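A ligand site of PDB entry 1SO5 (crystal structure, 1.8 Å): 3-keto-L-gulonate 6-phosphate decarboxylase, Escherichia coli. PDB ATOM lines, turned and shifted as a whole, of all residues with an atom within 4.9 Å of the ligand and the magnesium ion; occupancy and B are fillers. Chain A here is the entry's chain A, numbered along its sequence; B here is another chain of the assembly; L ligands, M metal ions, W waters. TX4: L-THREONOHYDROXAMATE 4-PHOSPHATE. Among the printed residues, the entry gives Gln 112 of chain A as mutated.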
ATOM      1  N   ALA A   9       1.865  28.222  11.496  1.00  0.00           N
ATOM      2  CA  ALA A   9       3.182  28.720  11.925  1.00  0.00           C
ATOM      3  C   ALA A   9       3.055  30.188  12.266  1.00  0.00           C
ATOM      4  O   ALA A   9       2.697  31.011  11.397  1.00  0.00           O
ATOM      5  CB  ALA A   9       4.248  28.501  10.850  1.00  0.00           C
ATOM      6  N   ASP A  11       5.095  32.805  12.537  1.00  0.00           N
ATOM      7  CA  ASP A  11       6.394  33.420  12.251  1.00  0.00           C
ATOM      8  C   ASP A  11       6.287  34.945  12.333  1.00  0.00           C
ATOM      9  O   ASP A  11       6.436  35.666  11.346  1.00  0.00           O
ATOM     10  CB  ASP A  11       6.915  32.947  10.913  1.00  0.00           C
ATOM     11  CG  ASP A  11       7.375  31.507  10.955  1.00  0.00           C
ATOM     12  OD1 ASP A  11       8.147  31.171  11.888  1.00  0.00           O
ATOM     13  OD2 ASP A  11       7.011  30.660  10.122  1.00  0.00           O
ATOM     14  N   GLU A  33       1.969  26.786  16.278  1.00  0.00           N
ATOM     15  CA  GLU A  33       3.421  26.820  16.323  1.00  0.00           C
ATOM     16  C   GLU A  33       3.878  28.233  16.718  1.00  0.00           C
ATOM     17  O   GLU A  33       3.505  29.246  16.101  1.00  0.00           O
ATOM     18  CB  GLU A  33       4.072  26.387  15.013  1.00  0.00           C
ATOM     19  CG  GLU A  33       5.484  26.950  14.769  1.00  0.00           C
ATOM     20  CD  GLU A  33       6.050  26.661  13.404  1.00  0.00           C
ATOM     21  OE1 GLU A  33       5.510  25.810  12.698  1.00  0.00           O
ATOM     22  OE2 GLU A  33       7.052  27.334  12.998  1.00  0.00           O
ATOM     23  N   GLY A  35       6.726  30.087  15.939  1.00  0.00           N
ATOM     24  CA  GLY A  35       7.760  30.055  14.940  1.00  0.00           C
ATOM     25  C   GLY A  35       9.125  30.427  15.495  1.00  0.00           C
ATOM     26  O   GLY A  35       9.239  31.101  16.509  1.00  0.00           O
ATOM     27  N   THR A  36      10.159  29.994  14.809  1.00  0.00           N
ATOM     28  CA  THR A  36      11.498  30.343  15.223  1.00  0.00           C
ATOM     29  C   THR A  36      11.671  31.874  15.309  1.00  0.00           C
ATOM     30  O   THR A  36      12.315  32.377  16.208  1.00  0.00           O
ATOM     31  CB  THR A  36      12.516  29.740  14.278  1.00  0.00           C
ATOM     32  OG1 THR A  36      12.192  28.371  13.983  1.00  0.00           O
ATOM     33  CG2 THR A  36      13.883  29.686  14.948  1.00  0.00           C
ATOM     34  N   ASP A  62       9.109  26.001  17.860  1.00  0.00           N
ATOM     35  CA  ASP A  62       9.993  25.739  16.730  1.00  0.00           C
ATOM     36  C   ASP A  62      11.341  26.413  16.992  1.00  0.00           C
ATOM     37  O   ASP A  62      11.746  27.382  16.293  1.00  0.00           O
ATOM     38  CB  ASP A  62       9.346  26.163  15.412  1.00  0.00           C
ATOM     39  CG  ASP A  62      10.081  25.680  14.186  1.00  0.00           C
ATOM     40  OD1 ASP A  62      11.120  24.942  14.275  1.00  0.00           O
ATOM     41  OD2 ASP A  62       9.712  26.034  13.046  1.00  0.00           O
ATOM     42  N   LYS A  64      14.334  24.973  16.788  1.00  0.00           N
ATOM     43  CA  LYS A  64      15.423  24.481  15.912  1.00  0.00           C
ATOM     44  C   LYS A  64      16.707  24.313  16.726  1.00  0.00           C
ATOM     45  O   LYS A  64      17.775  24.797  16.349  1.00  0.00           O
ATOM     46  CB  LYS A  64      15.620  25.403  14.685  1.00  0.00           C
ATOM     47  CG  LYS A  64      14.433  25.357  13.673  1.00  0.00           C
ATOM     48  CD  LYS A  64      14.671  26.253  12.474  1.00  0.00           C
ATOM     49  CE  LYS A  64      13.633  26.091  11.365  1.00  0.00           C
ATOM     50  NZ  LYS A  64      12.253  26.378  11.845  1.00  0.00           N
ATOM     51  N   GLN A 112      13.772  18.795  12.601  1.00  0.00           N
ATOM     52  CA  GLN A 112      13.435  19.728  11.534  1.00  0.00           C
ATOM     53  C   GLN A 112      14.428  19.525  10.397  1.00  0.00           C
ATOM     54  O   GLN A 112      15.631  19.738  10.576  1.00  0.00           O
ATOM     55  CB  GLN A 112      13.546  21.149  12.075  1.00  0.00           C
ATOM     56  CG  GLN A 112      13.208  22.212  11.057  1.00  0.00           C
ATOM     57  CD  GLN A 112      11.747  22.581  11.011  1.00  0.00           C
ATOM     58  OE1 GLN A 112      10.967  22.101  11.859  1.00  0.00           O
ATOM     59  NE2 GLN A 112      11.378  23.425  10.134  1.00  0.00           N
ATOM     60  N   HIS A 136      10.908  19.860   5.232  1.00  0.00           N
ATOM     61  CA  HIS A 136      10.752  21.305   5.030  1.00  0.00           C
ATOM     62  C   HIS A 136      11.498  21.784   3.793  1.00  0.00           C
ATOM     63  O   HIS A 136      12.738  21.627   3.666  1.00  0.00           O
ATOM     64  CB  HIS A 136      11.256  22.009   6.305  1.00  0.00           C
ATOM     65  CG  HIS A 136      11.313  23.507   6.220  1.00  0.00           C
ATOM     66  ND1 HIS A 136      10.373  24.279   5.566  1.00  0.00           N
ATOM     67  CD2 HIS A 136      12.168  24.372   6.800  1.00  0.00           C
ATOM     68  CE1 HIS A 136      10.693  25.562   5.703  1.00  0.00           C
ATOM     69  NE2 HIS A 136      11.770  25.640   6.454  1.00  0.00           N
ATOM     70  N   ARG A 139      12.331  28.327   3.025  1.00  0.00           N
ATOM     71  CA  ARG A 139      11.793  29.527   2.382  1.00  0.00           C
ATOM     72  C   ARG A 139      12.848  30.181   1.486  1.00  0.00           C
ATOM     73  O   ARG A 139      12.529  30.740   0.446  1.00  0.00           O
ATOM     74  CB  ARG A 139      11.203  30.472   3.449  1.00  0.00           C
ATOM     75  CG  ARG A 139      11.783  31.833   3.629  1.00  0.00           C
ATOM     76  CD  ARG A 139      11.369  32.484   4.947  1.00  0.00           C
ATOM     77  NE  ARG A 139      10.235  33.379   4.803  1.00  0.00           N
ATOM     78  CZ  ARG A 139       9.152  33.420   5.584  1.00  0.00           C
ATOM     79  NH1 ARG A 139       8.946  32.586   6.608  1.00  0.00           N
ATOM     80  NH2 ARG A 139       8.253  34.327   5.303  1.00  0.00           N
ATOM     81  N   THR A 169       6.001  20.845   5.132  1.00  0.00           N
ATOM     82  CA  THR A 169       5.957  22.303   5.259  1.00  0.00           C
ATOM     83  C   THR A 169       6.930  22.989   4.328  1.00  0.00           C
ATOM     84  O   THR A 169       7.968  22.417   3.948  1.00  0.00           O
ATOM     85  CB  THR A 169       6.222  22.722   6.721  1.00  0.00           C
ATOM     86  OG1 THR A 169       6.049  24.143   6.861  1.00  0.00           O
ATOM     87  CG2 THR A 169       7.675  22.400   7.120  1.00  0.00           C
ATOM     88  N   GLY A 170       6.642  24.239   3.986  1.00  0.00           N
ATOM     89  CA  GLY A 170       7.559  25.053   3.228  1.00  0.00           C
ATOM     90  C   GLY A 170       6.814  25.741   2.111  1.00  0.00           C
ATOM     91  O   GLY A 170       6.802  25.254   0.976  1.00  0.00           O
ATOM     92  N   GLY A 171       6.193  26.879   2.438  1.00  0.00           N
ATOM     93  CA  GLY A 171       5.432  27.675   1.500  1.00  0.00           C
ATOM     94  C   GLY A 171       4.263  26.936   0.888  1.00  0.00           C
ATOM     95  O   GLY A 171       3.866  27.227  -0.241  1.00  0.00           O
ATOM     96  N   LEU A 172       3.678  25.993   1.620  1.00  0.00           N
ATOM     97  CA  LEU A 172       2.542  25.252   1.085  1.00  0.00           C
ATOM     98  C   LEU A 172       1.371  26.179   0.771  1.00  0.00           C
ATOM     99  O   LEU A 172       1.024  27.045   1.579  1.00  0.00           O
ATOM    100  CB  LEU A 172       2.089  24.191   2.067  1.00  0.00           C
ATOM    101  CG  LEU A 172       3.001  22.974   2.258  1.00  0.00           C
ATOM    102  CD1 LEU A 172       2.418  22.108   3.355  1.00  0.00           C
ATOM    103  CD2 LEU A 172       3.130  22.185   0.980  1.00  0.00           C
ATOM    104  N   ILE A 189       1.879  22.023   7.716  1.00  0.00           N
ATOM    105  CA  ILE A 189       2.002  23.365   8.253  1.00  0.00           C
ATOM    106  C   ILE A 189       1.722  24.420   7.184  1.00  0.00           C
ATOM    107  O   ILE A 189       2.203  24.312   6.053  1.00  0.00           O
ATOM    108  CB  ILE A 189       3.417  23.594   8.757  1.00  0.00           C
ATOM    109  CG1 ILE A 189       3.836  22.511   9.766  1.00  0.00           C
ATOM    110  CG2 ILE A 189       3.511  24.981   9.336  1.00  0.00           C
ATOM    111  CD1 ILE A 189       5.243  22.675  10.266  1.00  0.00           C
ATOM    112  N   ALA A 190       0.964  25.457   7.536  1.00  0.00           N
ATOM    113  CA  ALA A 190       0.871  26.680   6.756  1.00  0.00           C
ATOM    114  C   ALA A 190       1.139  27.888   7.622  1.00  0.00           C
ATOM    115  O   ALA A 190       0.503  28.072   8.655  1.00  0.00           O
ATOM    116  CB  ALA A 190      -0.505  26.816   6.160  1.00  0.00           C
ATOM    117  N   GLY A 191       2.119  28.687   7.210  1.00  0.00           N
ATOM    118  CA  GLY A 191       2.425  29.972   7.794  1.00  0.00           C
ATOM    119  C   GLY A 191       1.851  31.067   6.924  1.00  0.00           C
ATOM    120  O   GLY A 191       0.729  31.508   7.138  1.00  0.00           O
ATOM    121  N   ARG A 192       2.627  31.512   5.951  1.00  0.00           N
ATOM    122  CA  ARG A 192       2.253  32.588   5.054  1.00  0.00           C
ATOM    123  C   ARG A 192       0.892  32.397   4.433  1.00  0.00           C
ATOM    124  O   ARG A 192       0.111  33.327   4.381  1.00  0.00           O
ATOM    125  CB  ARG A 192       3.310  32.779   3.971  1.00  0.00           C
ATOM    126  CG  ARG A 192       4.546  33.486   4.497  1.00  0.00           C
ATOM    127  CD  ARG A 192       5.693  33.408   3.518  1.00  0.00           C
ATOM    128  NE  ARG A 192       6.250  32.074   3.516  1.00  0.00           N
ATOM    129  CZ  ARG A 192       7.097  31.619   2.618  1.00  0.00           C
ATOM    130  NH1 ARG A 192       7.535  30.387   2.713  1.00  0.00           N
ATOM    131  NH2 ARG A 192       7.504  32.401   1.603  1.00  0.00           N
ATOM    132  N   ARG A 195      -1.616  33.200   7.425  1.00  0.00           N
ATOM    133  CA  ARG A 195      -1.470  34.512   8.028  1.00  0.00           C
ATOM    134  C   ARG A 195      -1.678  35.665   7.057  1.00  0.00           C
ATOM    135  O   ARG A 195      -2.235  36.679   7.432  1.00  0.00           O
ATOM    136  CB  ARG A 195      -0.070  34.695   8.627  1.00  0.00           C
ATOM    137  CG  ARG A 195       0.271  33.673   9.734  1.00  0.00           C
ATOM    138  CD  ARG A 195       1.425  34.172  10.629  1.00  0.00           C
ATOM    139  NE  ARG A 195       2.475  34.737   9.802  1.00  0.00           N
ATOM    140  CZ  ARG A 195       3.407  34.023   9.192  1.00  0.00           C
ATOM    141  NH1 ARG A 195       3.480  32.724   9.382  1.00  0.00           N
ATOM    142  NH2 ARG A 195       4.318  34.617   8.425  1.00  0.00           N
ATOM    143  N   ASP B  67      17.040  29.162   8.515  1.00  0.00           N
ATOM    144  CA  ASP B  67      16.220  29.519   7.348  1.00  0.00           C
ATOM    145  C   ASP B  67      15.729  30.937   7.571  1.00  0.00           C
ATOM    146  O   ASP B  67      15.929  31.490   8.660  1.00  0.00           O
ATOM    147  CB  ASP B  67      15.062  28.521   7.176  1.00  0.00           C
ATOM    148  CG  ASP B  67      14.290  28.724   5.881  1.00  0.00           C
ATOM    149  OD1 ASP B  67      14.853  29.270   4.888  1.00  0.00           O
ATOM    150  OD2 ASP B  67      13.091  28.416   5.778  1.00  0.00           O
HETATM  151  O7  TX4 L   1       6.616  28.473   4.744  1.00  0.00           O
HETATM  152  P   TX4 L   1       5.500  28.895   5.653  1.00  0.00           P
HETATM  153  O5  TX4 L   1       5.329  30.435   5.631  1.00  0.00           O
HETATM  154  O6  TX4 L   1       4.226  28.125   5.408  1.00  0.00           O
HETATM  155  O4  TX4 L   1       6.011  28.634   7.152  1.00  0.00           O
HETATM  156  C4  TX4 L   1       6.127  27.321   7.702  1.00  0.00           C
HETATM  157  C3  TX4 L   1       7.594  26.961   7.918  1.00  0.00           C
HETATM  158  O3  TX4 L   1       7.667  25.628   8.386  1.00  0.00           O
HETATM  159  C2  TX4 L   1       8.259  27.962   8.859  1.00  0.00           C
HETATM  160  O2  TX4 L   1       7.552  28.050  10.091  1.00  0.00           O
HETATM  161  C1  TX4 L   1       9.688  27.619   9.146  1.00  0.00           C
HETATM  162  O1  TX4 L   1       9.942  26.876  10.213  1.00  0.00           O
HETATM  163  N   TX4 L   1      10.581  28.065   8.381  1.00  0.00           N
HETATM  164  ON  TX4 L   1      11.947  27.811   8.644  1.00  0.00           O
HETATM  165 MG    MG M   1       8.524  27.035  11.750  1.00  0.00          MG
HETATM  166  O   HOH W   1       7.544  25.198  11.058  1.00  0.00           O
HETATM  167  O   HOH W   2       2.440  28.911   3.536  1.00  0.00           O
HETATM  168  O   HOH W   3      10.418  29.596   6.403  1.00  0.00           O
HETATM  169  O   HOH W   4       5.839  31.742   7.956  1.00  0.00           O
HETATM  170  O   HOH W   5       4.070  25.669   4.480  1.00  0.00           O
HETATM  171  O   HOH W   6       9.444  28.922  12.208  1.00  0.00           O
HETATM  172  O   HOH W   7       9.270  27.973   4.769  1.00  0.00           O
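Merely in contact with the ligand: Ala 9 (3.4 Å), Gln 112 (3.7 Å), Gly 170 (3.8 Å), Ile 189 (3.9 Å) and Ala 190 (3.8 Å).
Hydrophobic or aromatic side chains within 4 Å of the ligand: Ala 9, His 136 and Ile 189.
Of the 20 residues printed, 15 come within 4 Å of the ligand.
An oxygen (O1) of the ligand sits close to the side-chain amino group of Lys 64 (2.9 Å).
ON of the ligand sits at hydrogen-bond distance from NE2 of His 136, 3.1 Å away.
O5 of the ligand is in salt-bridge range of NE of Arg 192 (2.8 Å).
The backbone NH of Arg 192 sits at hydrogen-bond distance from an oxygen (O5) of the ligand (2.9 Å).
OD2 of Asp 67 of chain B sits at hydrogen-bond distance from ON of the ligand, 3.1 Å away.
An oxygen (O6) of the ligand lies within hydrogen-bond range of the backbone NH of Gly 191 (2.8 Å).
The backbone NH (N) of Gly 171 is in hydrogen-bond range of an oxygen (O7) of the ligand.
The side-chain carboxylate of Asp 11 lies close to an oxygen (O2) of the ligand (2.7 Å).
The side-chain hydroxyl of Thr 169 is in hydrogen-bond range of an oxygen (O3) of the ligand (2.7 Å).
NH1 of Arg 195 sits at hydrogen-bond distance from O of Ala 9 (2.8 Å).
The backbone NH of Ala 9 lies within hydrogen-bond range of the backbone carbonyl oxygen of Ala 190.
A ring nitrogen (NE2) of His 136 sits at hydrogen-bond distance from the side-chain carboxylate (OD2) of Asp 67 of chain B (3.1 Å).
The side-chain hydroxyl (OG1) of Thr 36 sits at hydrogen-bond distance from the side-chain amino group (NZ) of Lys 64 (2.9 Å).
The backbone carbonyl oxygen of Asp 62 lies within hydrogen-bond range of the side-chain hydroxyl of Thr 36, at 2.6 Å.
The backbone NH (N) of Arg 139 sits at hydrogen-bond distance from the side-chain carboxylate (OD2) of Asp 67 of chain B (2.9 Å).
The side-chain amino group of Lys 64 is in salt-bridge range of the side-chain carboxylate of Asp 62, at 3.0 Å.
O of Thr 169 lies close to ND1 of His 136 (3.4 Å).
The magnesium ion is bound by OE2 of Glu 33 (2.0 Å), OD2 of Asp 62 (2.0 Å), O1 of the ligand (2.1 Å), water W6 (2.1 Å), O2 of the ligand (2.2 Å) and water W1 (2.2 Å).
Water W6 bridges OD1 of Asp 11 (2.6 Å) and N of Thr 36 (2.9 Å).
Water W1 bridges the side-chain carboxylate (OE1) of Glu 33 and an oxygen (O3) of the ligand.
Water W3 lies within hydrogen-bond range of N of the ligand (2.5 Å), OD2 of Asp 67 of chain B (3.0 Å) and NH1 of Arg 139 (3.3 Å).
Water W2 lies within hydrogen-bond range of O6 of the ligand (2.7 Å) and O of Leu 172 (3.1 Å).
Water W4 lies within hydrogen-bond range of the side-chain carboxylate (OD2) of Asp 11 (2.7 Å), an oxygen (O5) of the ligand (2.7 Å), the guanidinium group (NH1) of Arg 195 (2.9 Å) and the guanidinium group (NH1) of Arg 139 (3.5 Å).
Lys 64 touches the magnesium ion.
Three residues have an atom within 4 Å of the magnesium ion: Glu 33, Asp 62 and Lys 64.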
